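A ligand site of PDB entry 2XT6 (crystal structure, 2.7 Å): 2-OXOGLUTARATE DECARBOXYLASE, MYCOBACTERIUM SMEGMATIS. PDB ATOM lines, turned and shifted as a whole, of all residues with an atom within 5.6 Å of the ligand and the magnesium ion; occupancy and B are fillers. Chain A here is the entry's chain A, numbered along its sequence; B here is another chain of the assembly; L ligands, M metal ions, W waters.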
ATOM      1  N   HIS A 425      -7.792  -9.036 -12.749  1.00  0.00           N
ATOM      2  CA  HIS A 425      -6.843  -8.621 -13.792  1.00  0.00           C
ATOM      3  C   HIS A 425      -6.010  -7.374 -13.416  1.00  0.00           C
ATOM      4  O   HIS A 425      -4.869  -7.265 -13.889  1.00  0.00           O
ATOM      5  CB  HIS A 425      -7.600  -8.331 -15.107  1.00  0.00           C
ATOM      6  CG  HIS A 425      -8.669  -7.281 -14.957  1.00  0.00           C
ATOM      7  ND1 HIS A 425      -8.552  -6.033 -15.567  1.00  0.00           N
ATOM      8  CD2 HIS A 425      -9.833  -7.326 -14.271  1.00  0.00           C
ATOM      9  CE1 HIS A 425      -9.645  -5.364 -15.237  1.00  0.00           C
ATOM     10  NE2 HIS A 425     -10.437  -6.096 -14.442  1.00  0.00           N
ATOM     11  N   ARG A 426      -6.571  -6.438 -12.601  1.00  0.00           N
ATOM     12  CA  ARG A 426      -5.888  -5.194 -12.213  1.00  0.00           C
ATOM     13  C   ARG A 426      -4.515  -5.438 -11.550  1.00  0.00           C
ATOM     14  O   ARG A 426      -4.437  -5.903 -10.395  1.00  0.00           O
ATOM     15  CB  ARG A 426      -6.752  -4.285 -11.317  1.00  0.00           C
ATOM     16  CG  ARG A 426      -6.191  -2.864 -11.249  1.00  0.00           C
ATOM     17  CD  ARG A 426      -7.056  -1.850 -10.506  1.00  0.00           C
ATOM     18  NE  ARG A 426      -8.364  -1.622 -11.120  1.00  0.00           N
ATOM     19  CZ  ARG A 426      -8.598  -0.903 -12.210  1.00  0.00           C
ATOM     20  NH1 ARG A 426      -7.601  -0.322 -12.866  1.00  0.00           N
ATOM     21  NH2 ARG A 426      -9.837  -0.757 -12.664  1.00  0.00           N
ATOM     22  N   SER A 490     -13.070 -13.707 -16.021  1.00  0.00           N
ATOM     23  CA  SER A 490     -13.366 -12.295 -15.861  1.00  0.00           C
ATOM     24  C   SER A 490     -14.447 -12.126 -14.802  1.00  0.00           C
ATOM     25  O   SER A 490     -14.656 -11.004 -14.340  1.00  0.00           O
ATOM     26  CB  SER A 490     -13.776 -11.669 -17.191  1.00  0.00           C
ATOM     27  OG  SER A 490     -12.716 -11.754 -18.128  1.00  0.00           O
ATOM     28  N   HIS A 491     -15.120 -13.229 -14.397  1.00  0.00           N
ATOM     29  CA  HIS A 491     -16.127 -13.259 -13.313  1.00  0.00           C
ATOM     30  C   HIS A 491     -15.447 -13.024 -12.009  1.00  0.00           C
ATOM     31  O   HIS A 491     -14.749 -13.922 -11.494  1.00  0.00           O
ATOM     32  CB  HIS A 491     -16.862 -14.597 -13.272  1.00  0.00           C
ATOM     33  CG  HIS A 491     -17.728 -14.809 -14.450  1.00  0.00           C
ATOM     34  ND1 HIS A 491     -17.228 -14.738 -15.735  1.00  0.00           N
ATOM     35  CD2 HIS A 491     -19.052 -15.104 -14.501  1.00  0.00           C
ATOM     36  CE1 HIS A 491     -18.270 -14.937 -16.527  1.00  0.00           C
ATOM     37  NE2 HIS A 491     -19.377 -15.182 -15.814  1.00  0.00           N
ATOM     38  N   LEU A 492     -15.588 -11.792 -11.491  1.00  0.00           N
ATOM     39  CA  LEU A 492     -14.944 -11.320 -10.269  1.00  0.00           C
ATOM     40  C   LEU A 492     -15.318 -12.166  -9.063  1.00  0.00           C
ATOM     41  O   LEU A 492     -16.488 -12.561  -8.883  1.00  0.00           O
ATOM     42  CB  LEU A 492     -15.259  -9.827 -10.019  1.00  0.00           C
ATOM     43  CG  LEU A 492     -14.712  -8.866 -11.102  1.00  0.00           C
ATOM     44  CD1 LEU A 492     -15.448  -7.544 -11.093  1.00  0.00           C
ATOM     45  CD2 LEU A 492     -13.229  -8.658 -10.972  1.00  0.00           C
ATOM     46  N   GLY A 530     -11.204  -6.330  -5.468  1.00  0.00           N
ATOM     47  CA  GLY A 530     -11.506  -4.924  -5.706  1.00  0.00           C
ATOM     48  C   GLY A 530     -12.595  -4.582  -4.721  1.00  0.00           C
ATOM     49  O   GLY A 530     -13.278  -5.483  -4.223  1.00  0.00           O
ATOM     50  N   ASP A 531     -12.777  -3.280  -4.430  1.00  0.00           N
ATOM     51  CA  ASP A 531     -13.755  -2.834  -3.429  1.00  0.00           C
ATOM     52  C   ASP A 531     -15.218  -3.156  -3.773  1.00  0.00           C
ATOM     53  O   ASP A 531     -15.943  -3.623  -2.895  1.00  0.00           O
ATOM     54  CB  ASP A 531     -13.598  -1.337  -3.115  1.00  0.00           C
ATOM     55  CG  ASP A 531     -13.836  -0.331  -4.220  1.00  0.00           C
ATOM     56  OD1 ASP A 531     -13.060  -0.335  -5.194  1.00  0.00           O
ATOM     57  OD2 ASP A 531     -14.716   0.573  -4.022  1.00  0.00           O
ATOM     58  N   ALA A 532     -15.657  -2.920  -5.027  1.00  0.00           N
ATOM     59  CA  ALA A 532     -17.062  -3.187  -5.393  1.00  0.00           C
ATOM     60  C   ALA A 532     -17.417  -4.700  -5.437  1.00  0.00           C
ATOM     61  O   ALA A 532     -18.468  -5.085  -4.946  1.00  0.00           O
ATOM     62  CB  ALA A 532     -17.391  -2.543  -6.713  1.00  0.00           C
ATOM     63  N   ALA A 533     -16.521  -5.543  -5.993  1.00  0.00           N
ATOM     64  CA  ALA A 533     -16.740  -6.966  -6.125  1.00  0.00           C
ATOM     65  C   ALA A 533     -16.745  -7.656  -4.751  1.00  0.00           C
ATOM     66  O   ALA A 533     -17.614  -8.488  -4.485  1.00  0.00           O
ATOM     67  CB  ALA A 533     -15.684  -7.561  -7.046  1.00  0.00           C
ATOM     68  N   PHE A 534     -15.834  -7.244  -3.841  1.00  0.00           N
ATOM     69  CA  PHE A 534     -15.752  -7.826  -2.497  1.00  0.00           C
ATOM     70  C   PHE A 534     -17.055  -7.634  -1.709  1.00  0.00           C
ATOM     71  O   PHE A 534     -17.463  -8.549  -0.987  1.00  0.00           O
ATOM     72  CB  PHE A 534     -14.564  -7.225  -1.711  1.00  0.00           C
ATOM     73  CG  PHE A 534     -14.171  -8.017  -0.486  1.00  0.00           C
ATOM     74  CD1 PHE A 534     -13.438  -9.197  -0.601  1.00  0.00           C
ATOM     75  CD2 PHE A 534     -14.538  -7.579   0.789  1.00  0.00           C
ATOM     76  CE1 PHE A 534     -13.065  -9.915   0.540  1.00  0.00           C
ATOM     77  CE2 PHE A 534     -14.180  -8.326   1.928  1.00  0.00           C
ATOM     78  CZ  PHE A 534     -13.446  -9.476   1.800  1.00  0.00           C
ATOM     79  N   GLN A 537     -20.427  -9.432  -4.292  1.00  0.00           N
ATOM     80  CA  GLN A 537     -20.454 -10.852  -4.702  1.00  0.00           C
ATOM     81  C   GLN A 537     -20.599 -11.820  -3.508  1.00  0.00           C
ATOM     82  O   GLN A 537     -19.736 -11.849  -2.629  1.00  0.00           O
ATOM     83  CB  GLN A 537     -19.221 -11.204  -5.547  1.00  0.00           C
ATOM     84  CG  GLN A 537     -19.185 -10.553  -6.937  1.00  0.00           C
ATOM     85  CD  GLN A 537     -20.092 -11.195  -7.951  1.00  0.00           C
ATOM     86  OE1 GLN A 537     -19.958 -12.373  -8.284  1.00  0.00           O
ATOM     87  NE2 GLN A 537     -21.012 -10.418  -8.505  1.00  0.00           N
ATOM     88  N   VAL A 562      -7.846  -3.976  -2.936  1.00  0.00           N
ATOM     89  CA  VAL A 562      -7.340  -2.812  -3.671  1.00  0.00           C
ATOM     90  C   VAL A 562      -8.583  -1.898  -3.820  1.00  0.00           C
ATOM     91  O   VAL A 562      -9.360  -2.027  -4.761  1.00  0.00           O
ATOM     92  CB  VAL A 562      -6.680  -3.224  -5.017  1.00  0.00           C
ATOM     93  CG1 VAL A 562      -6.151  -2.012  -5.782  1.00  0.00           C
ATOM     94  CG2 VAL A 562      -5.567  -4.268  -4.803  1.00  0.00           C
ATOM     95  N   ASN A 563      -8.834  -1.118  -2.769  1.00  0.00           N
ATOM     96  CA  ASN A 563      -9.988  -0.233  -2.651  1.00  0.00           C
ATOM     97  C   ASN A 563      -9.673   1.170  -3.211  1.00  0.00           C
ATOM     98  O   ASN A 563      -9.249   2.069  -2.471  1.00  0.00           O
ATOM     99  CB  ASN A 563     -10.355  -0.185  -1.179  1.00  0.00           C
ATOM    100  CG  ASN A 563     -11.473   0.715  -0.769  1.00  0.00           C
ATOM    101  OD1 ASN A 563     -12.241   1.253  -1.572  1.00  0.00           O
ATOM    102  ND2 ASN A 563     -11.602   0.869   0.539  1.00  0.00           N
ATOM    103  N   ASN A 564      -9.888   1.349  -4.535  1.00  0.00           N
ATOM    104  CA  ASN A 564      -9.678   2.602  -5.255  1.00  0.00           C
ATOM    105  C   ASN A 564     -10.931   3.501  -5.181  1.00  0.00           C
ATOM    106  O   ASN A 564     -11.066   4.449  -5.952  1.00  0.00           O
ATOM    107  CB  ASN A 564      -9.280   2.322  -6.691  1.00  0.00           C
ATOM    108  CG  ASN A 564     -10.064   1.258  -7.419  1.00  0.00           C
ATOM    109  OD1 ASN A 564     -11.206   0.939  -7.096  1.00  0.00           O
ATOM    110  ND2 ASN A 564      -9.483   0.735  -8.488  1.00  0.00           N
ATOM    111  N   GLN A 565     -11.846   3.200  -4.228  1.00  0.00           N
ATOM    112  CA  GLN A 565     -13.060   3.946  -3.891  1.00  0.00           C
ATOM    113  C   GLN A 565     -14.002   4.218  -5.137  1.00  0.00           C
ATOM    114  O   GLN A 565     -14.741   5.214  -5.205  1.00  0.00           O
ATOM    115  CB  GLN A 565     -12.637   5.261  -3.212  1.00  0.00           C
ATOM    116  CG  GLN A 565     -11.600   5.063  -2.113  1.00  0.00           C
ATOM    117  CD  GLN A 565     -11.084   6.363  -1.558  1.00  0.00           C
ATOM    118  OE1 GLN A 565     -11.848   7.163  -1.001  1.00  0.00           O
ATOM    119  NE2 GLN A 565      -9.778   6.579  -1.672  1.00  0.00           N
ATOM    120  N   ILE A 566     -13.966   3.264  -6.089  1.00  0.00           N
ATOM    121  CA  ILE A 566     -14.685   3.308  -7.364  1.00  0.00           C
ATOM    122  C   ILE A 566     -14.844   1.872  -7.926  1.00  0.00           C
ATOM    123  O   ILE A 566     -13.963   1.020  -7.745  1.00  0.00           O
ATOM    124  CB  ILE A 566     -13.939   4.266  -8.384  1.00  0.00           C
ATOM    125  CG1 ILE A 566     -14.812   4.687  -9.599  1.00  0.00           C
ATOM    126  CG2 ILE A 566     -12.557   3.759  -8.851  1.00  0.00           C
ATOM    127  CD1 ILE A 566     -15.754   5.711  -9.309  1.00  0.00           C
ATOM    128  N   GLY A 567     -15.962   1.664  -8.623  1.00  0.00           N
ATOM    129  CA  GLY A 567     -16.289   0.410  -9.289  1.00  0.00           C
ATOM    130  C   GLY A 567     -16.768   0.755 -10.687  1.00  0.00           C
ATOM    131  O   GLY A 567     -17.969   0.966 -10.901  1.00  0.00           O
ATOM    132  N   PHE A 568     -15.805   0.865 -11.631  1.00  0.00           N
ATOM    133  CA  PHE A 568     -16.026   1.267 -13.026  1.00  0.00           C
ATOM    134  C   PHE A 568     -16.556   2.729 -13.070  1.00  0.00           C
ATOM    135  O   PHE A 568     -15.765   3.672 -13.124  1.00  0.00           O
ATOM    136  CB  PHE A 568     -16.942   0.269 -13.764  1.00  0.00           C
ATOM    137  CG  PHE A 568     -17.063   0.390 -15.271  1.00  0.00           C
ATOM    138  CD1 PHE A 568     -16.778   1.609 -15.912  1.00  0.00           C
ATOM    139  CD2 PHE A 568     -17.513  -0.671 -16.040  1.00  0.00           C
ATOM    140  CE1 PHE A 568     -16.897   1.723 -17.300  1.00  0.00           C
ATOM    141  CE2 PHE A 568     -17.680  -0.539 -17.425  1.00  0.00           C
ATOM    142  CZ  PHE A 568     -17.363   0.652 -18.057  1.00  0.00           C
ATOM    143  N   ARG A 629      -7.835   5.149  -8.631  1.00  0.00           N
ATOM    144  CA  ARG A 629      -7.664   4.713  -9.999  1.00  0.00           C
ATOM    145  C   ARG A 629      -7.403   5.997 -10.774  1.00  0.00           C
ATOM    146  O   ARG A 629      -8.335   6.793 -10.927  1.00  0.00           O
ATOM    147  CB  ARG A 629      -8.929   3.979 -10.445  1.00  0.00           C
ATOM    148  CG  ARG A 629      -8.733   3.009 -11.595  1.00  0.00           C
ATOM    149  CD  ARG A 629     -10.069   2.687 -12.227  1.00  0.00           C
ATOM    150  NE  ARG A 629     -10.716   3.912 -12.708  1.00  0.00           N
ATOM    151  CZ  ARG A 629     -12.023   4.047 -12.874  1.00  0.00           C
ATOM    152  NH1 ARG A 629     -12.837   3.037 -12.644  1.00  0.00           N
ATOM    153  NH2 ARG A 629     -12.523   5.206 -13.276  1.00  0.00           N
ATOM    154  N   HIS A 633     -11.676   3.720 -16.645  1.00  0.00           N
ATOM    155  CA  HIS A 633     -11.845   2.297 -16.472  1.00  0.00           C
ATOM    156  C   HIS A 633     -11.290   1.558 -17.656  1.00  0.00           C
ATOM    157  O   HIS A 633     -10.652   0.533 -17.460  1.00  0.00           O
ATOM    158  CB  HIS A 633     -13.313   1.907 -16.241  1.00  0.00           C
ATOM    159  CG  HIS A 633     -13.453   0.479 -15.799  1.00  0.00           C
ATOM    160  ND1 HIS A 633     -13.161   0.093 -14.493  1.00  0.00           N
ATOM    161  CD2 HIS A 633     -13.814  -0.613 -16.515  1.00  0.00           C
ATOM    162  CE1 HIS A 633     -13.363  -1.222 -14.456  1.00  0.00           C
ATOM    163  NE2 HIS A 633     -13.748  -1.690 -15.653  1.00  0.00           N
ATOM    164  N   GLN B 787     -25.357  -2.853 -13.874  1.00  0.00           N
ATOM    165  CA  GLN B 787     -24.019  -2.330 -13.536  1.00  0.00           C
ATOM    166  C   GLN B 787     -23.650  -1.209 -14.489  1.00  0.00           C
ATOM    167  O   GLN B 787     -23.629  -1.417 -15.704  1.00  0.00           O
ATOM    168  CB  GLN B 787     -22.972  -3.441 -13.550  1.00  0.00           C
ATOM    169  CG  GLN B 787     -22.840  -4.175 -12.223  1.00  0.00           C
ATOM    170  CD  GLN B 787     -22.598  -5.641 -12.433  1.00  0.00           C
ATOM    171  OE1 GLN B 787     -21.860  -6.064 -13.326  1.00  0.00           O
ATOM    172  NE2 GLN B 787     -23.217  -6.466 -11.610  1.00  0.00           N
ATOM    173  N   ASP B 788     -23.418   0.003 -13.929  1.00  0.00           N
ATOM    174  CA  ASP B 788     -23.056   1.217 -14.667  1.00  0.00           C
ATOM    175  C   ASP B 788     -24.107   1.535 -15.771  1.00  0.00           C
ATOM    176  O   ASP B 788     -23.741   2.020 -16.838  1.00  0.00           O
ATOM    177  CB  ASP B 788     -21.635   1.077 -15.247  1.00  0.00           C
ATOM    178  CG  ASP B 788     -20.615   0.602 -14.220  1.00  0.00           C
ATOM    179  OD1 ASP B 788     -20.257   1.394 -13.337  1.00  0.00           O
ATOM    180  OD2 ASP B 788     -20.268  -0.603 -14.249  1.00  0.00           O
ATOM    181  N   LEU B 836     -22.376  -4.657  -7.360  1.00  0.00           N
ATOM    182  CA  LEU B 836     -21.712  -5.639  -8.217  1.00  0.00           C
ATOM    183  C   LEU B 836     -22.173  -7.057  -7.877  1.00  0.00           C
ATOM    184  O   LEU B 836     -21.425  -7.871  -7.333  1.00  0.00           O
ATOM    185  CB  LEU B 836     -20.178  -5.519  -8.153  1.00  0.00           C
ATOM    186  CG  LEU B 836     -19.451  -5.667  -9.470  1.00  0.00           C
ATOM    187  CD1 LEU B 836     -18.050  -5.139  -9.363  1.00  0.00           C
ATOM    188  CD2 LEU B 836     -19.451  -7.109  -9.973  1.00  0.00           C
ATOM    189  N   GLU B 838     -25.201 -10.206  -9.518  1.00  0.00           N
ATOM    190  CA  GLU B 838     -26.069 -10.626 -10.629  1.00  0.00           C
ATOM    191  C   GLU B 838     -27.295 -11.329 -10.075  1.00  0.00           C
ATOM    192  O   GLU B 838     -28.405 -11.019 -10.469  1.00  0.00           O
ATOM    193  CB  GLU B 838     -25.344 -11.503 -11.667  1.00  0.00           C
ATOM    194  CG  GLU B 838     -24.359 -10.737 -12.538  1.00  0.00           C
ATOM    195  CD  GLU B 838     -23.054 -10.290 -11.895  1.00  0.00           C
ATOM    196  OE1 GLU B 838     -22.566  -9.178 -12.229  1.00  0.00           O
ATOM    197  OE2 GLU B 838     -22.495 -11.057 -11.071  1.00  0.00           O
ATOM    198  N   GLN B 862     -23.707  -6.286 -17.575  1.00  0.00           N
ATOM    199  CA  GLN B 862     -22.570  -5.494 -18.030  1.00  0.00           C
ATOM    200  C   GLN B 862     -22.179  -6.082 -19.404  1.00  0.00           C
ATOM    201  O   GLN B 862     -22.072  -5.369 -20.410  1.00  0.00           O
ATOM    202  CB  GLN B 862     -21.448  -5.552 -16.981  1.00  0.00           C
ATOM    203  CG  GLN B 862     -20.188  -4.807 -17.402  1.00  0.00           C
ATOM    204  CD  GLN B 862     -19.891  -3.672 -16.491  1.00  0.00           C
ATOM    205  OE1 GLN B 862     -18.887  -3.676 -15.802  1.00  0.00           O
ATOM    206  NE2 GLN B 862     -20.745  -2.657 -16.481  1.00  0.00           N
ATOM    207  N   PHE B 866     -22.035 -12.484 -17.795  1.00  0.00           N
ATOM    208  CA  PHE B 866     -22.055 -12.507 -16.343  1.00  0.00           C
ATOM    209  C   PHE B 866     -23.408 -12.914 -15.759  1.00  0.00           C
ATOM    210  O   PHE B 866     -23.438 -13.282 -14.567  1.00  0.00           O
ATOM    211  CB  PHE B 866     -21.576 -11.153 -15.777  1.00  0.00           C
ATOM    212  CG  PHE B 866     -20.163 -10.824 -16.233  1.00  0.00           C
ATOM    213  CD1 PHE B 866     -19.905  -9.715 -17.034  1.00  0.00           C
ATOM    214  CD2 PHE B 866     -19.103 -11.659 -15.888  1.00  0.00           C
ATOM    215  CE1 PHE B 866     -18.613  -9.438 -17.466  1.00  0.00           C
ATOM    216  CE2 PHE B 866     -17.798 -11.384 -16.359  1.00  0.00           C
ATOM    217  CZ  PHE B 866     -17.566 -10.267 -17.123  1.00  0.00           C
ATOM    218  N   HIS B 906     -16.559 -11.921 -22.674  1.00  0.00           N
ATOM    219  CA  HIS B 906     -17.060 -10.662 -23.242  1.00  0.00           C
ATOM    220  C   HIS B 906     -17.606 -10.943 -24.630  1.00  0.00           C
ATOM    221  O   HIS B 906     -17.390 -10.137 -25.537  1.00  0.00           O
ATOM    222  CB  HIS B 906     -15.953  -9.587 -23.245  1.00  0.00           C
ATOM    223  CG  HIS B 906     -15.367  -9.343 -21.883  1.00  0.00           C
ATOM    224  ND1 HIS B 906     -15.964  -8.440 -20.998  1.00  0.00           N
ATOM    225  CD2 HIS B 906     -14.343  -9.967 -21.248  1.00  0.00           C
ATOM    226  CE1 HIS B 906     -15.249  -8.507 -19.883  1.00  0.00           C
ATOM    227  NE2 HIS B 906     -14.277  -9.425 -19.989  1.00  0.00           N
HETATM  228  N1  LIG L   1     -19.683  -9.278 -12.768  1.00  0.00           N
HETATM  229  C1  LIG L   1     -18.676 -10.123 -12.592  1.00  0.00           C
HETATM  230  C2  LIG L   1     -18.793 -11.364 -11.753  1.00  0.00           C
HETATM  231  N2  LIG L   1     -17.517  -9.907 -13.165  1.00  0.00           N
HETATM  232  C3  LIG L   1     -17.302  -8.843 -13.905  1.00  0.00           C
HETATM  233  N3  LIG L   1     -16.052  -8.753 -14.462  1.00  0.00           N
HETATM  234  C4  LIG L   1     -18.326  -7.888 -14.111  1.00  0.00           C
HETATM  235  C5  LIG L   1     -19.547  -8.168 -13.513  1.00  0.00           C
HETATM  236  C6  LIG L   1     -18.108  -6.617 -14.916  1.00  0.00           C
HETATM  237  N4  LIG L   1     -17.078  -5.735 -14.330  1.00  0.00           N
HETATM  238  C7  LIG L   1     -15.859  -5.683 -14.769  1.00  0.00           C
HETATM  239  S1  LIG L   1     -14.914  -4.497 -13.920  1.00  0.00           S
HETATM  240  C8  LIG L   1     -16.319  -4.117 -12.920  1.00  0.00           C
HETATM  241  C9  LIG L   1     -17.332  -4.899 -13.326  1.00  0.00           C
HETATM  242  C10 LIG L   1     -18.666  -4.714 -12.672  1.00  0.00           C
HETATM  243  C11 LIG L   1     -16.261  -3.132 -11.780  1.00  0.00           C
HETATM  244  C12 LIG L   1     -15.187  -3.606 -10.789  1.00  0.00           C
HETATM  245  O1  LIG L   1     -15.239  -2.897  -9.546  1.00  0.00           O
HETATM  246  P1  LIG L   1     -14.118  -3.172  -8.420  1.00  0.00           P
HETATM  247  O2  LIG L   1     -14.419  -4.459  -7.756  1.00  0.00           O
HETATM  248  O3  LIG L   1     -14.052  -2.017  -7.314  1.00  0.00           O
HETATM  249  O4  LIG L   1     -12.686  -3.272  -9.141  1.00  0.00           O
HETATM  250  P2  LIG L   1     -11.713  -2.295  -9.770  1.00  0.00           P
HETATM  251  O5  LIG L   1     -11.700  -2.562 -11.360  1.00  0.00           O
HETATM  252  O6  LIG L   1     -12.121  -0.913  -9.473  1.00  0.00           O
HETATM  253  O7  LIG L   1     -10.231  -2.533  -9.165  1.00  0.00           O
HETATM  254 MG    MG M   1     -12.606  -0.616  -7.205  1.00  0.00          MG
HETATM  255  O   HOH W   1     -11.067  -1.824  -6.699  1.00  0.00           O
HETATM  256  O   HOH W   2     -12.406  -6.495  -8.543  1.00  0.00           O
HETATM  257  O   HOH W   3     -12.936   0.373 -11.678  1.00  0.00           O
HETATM  258  O   HOH W   4     -14.676  -7.549 -17.137  1.00  0.00           O
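The magnesium ion is bound by O3 of the ligand (2.0 Å).
The magnesium ion is bound by water W1 (2.0 Å).
The side-chain carboxylate (OD1) of Asp 531 binds the magnesium ion (2.1 Å).
The side-chain amide oxygen (OD1) of Asn 564 is bound to the magnesium ion (2.1 Å).
The magnesium ion is bound by O of Ile 566.
O6 of the ligand binds the magnesium ion, 2.3 Å away.
The magnesium ion has six donor atoms within binding distance.
A nitrogen (N2) of the ligand sits at hydrogen-bond distance from the backbone NH (N) of Leu 492 (3.2 Å).
The backbone NH (N) of Ala 533 lies within hydrogen-bond range of an oxygen (O2) of the ligand, 2.9 Å away.
The guanidinium group (NE) of Arg 426 is in salt-bridge range of an oxygen (O7) of the ligand (2.9 Å).
The backbone carbonyl oxygen (O) of Ser 490 is in hydrogen-bond range of a nitrogen (N3) of the ligand (2.7 Å).
A sulfur (S1) of the ligand sits close to a ring nitrogen (NE2) of His 633, at 3.5 Å.
O3 of the ligand lies close to N of Asp 531 (3.4 Å).
The backbone NH of Ala 532 is in hydrogen-bond range of an oxygen (O2) of the ligand (3.4 Å).
Water W1 lies within hydrogen-bond range of the backbone carbonyl oxygen of Val 562, an oxygen (O7) of the ligand and the backbone NH of Asp 531.
Water W2 bridges O2 of the ligand and N of Gly 530.
Water W4 lies within hydrogen-bond range of N3 of the ligand and NE2 of His 906 of chain B.
OE2 of Glu 838 of chain B is in hydrogen-bond range of NE2 of Gln 537 (3.0 Å).
The side-chain amide nitrogen (NE2) of Gln 537 sits at hydrogen-bond distance from the backbone carbonyl oxygen (O) of Leu 836 of chain B (2.8 Å).
NE2 of His 906 of chain B sits at hydrogen-bond distance from OG of Ser 490.
ND1 of His 633 sits at hydrogen-bond distance from NH1 of Arg 629.
The side-chain amide nitrogen of Gln 862 of chain B lies within hydrogen-bond range of the side-chain carboxylate of Asp 788 of chain B, 3.1 Å away.
NE2 of Gln 862 of chain B is in hydrogen-bond range of O of Gln 787 of chain B.
The side-chain amide nitrogen (NE2) of Gln 787 of chain B sits at hydrogen-bond distance from the side-chain carboxylate (OE1) of Glu 838 of chain B, 2.9 Å away.
The backbone carbonyl oxygen (O) of Phe 568 lies within hydrogen-bond range of the guanidinium group (NH1) of Arg 629 (3.0 Å).
The side-chain carboxylate (OE1) of Glu 838 of chain B sits close to a nitrogen (N1) of the ligand, at 2.9 Å.
A nitrogen (N4) of the ligand lies close to the side-chain amide oxygen of Gln 862 of chain B.
Merely in contact with the ligand: Gln 787 of chain B, Leu 836 of chain B, Phe 866 of chain B, Gly 567, Gly 530, His 491, Gln 537 and Phe 568.
Hydrophobic or aromatic side chains that line the ligand: Leu 492, Ala 532, Ala 533, Phe 568, His 633, Leu 836 of chain B and Phe 866 of chain B.
The nearest printed residue that does not touch the ligand is Val 562 (4.5 Å).
Within 4 Å of the magnesium ion: Asp 531, Asn 564 and Ile 566.
The nearest printed residue that does not touch the magnesium ion is Gly 567 (4.3 Å).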
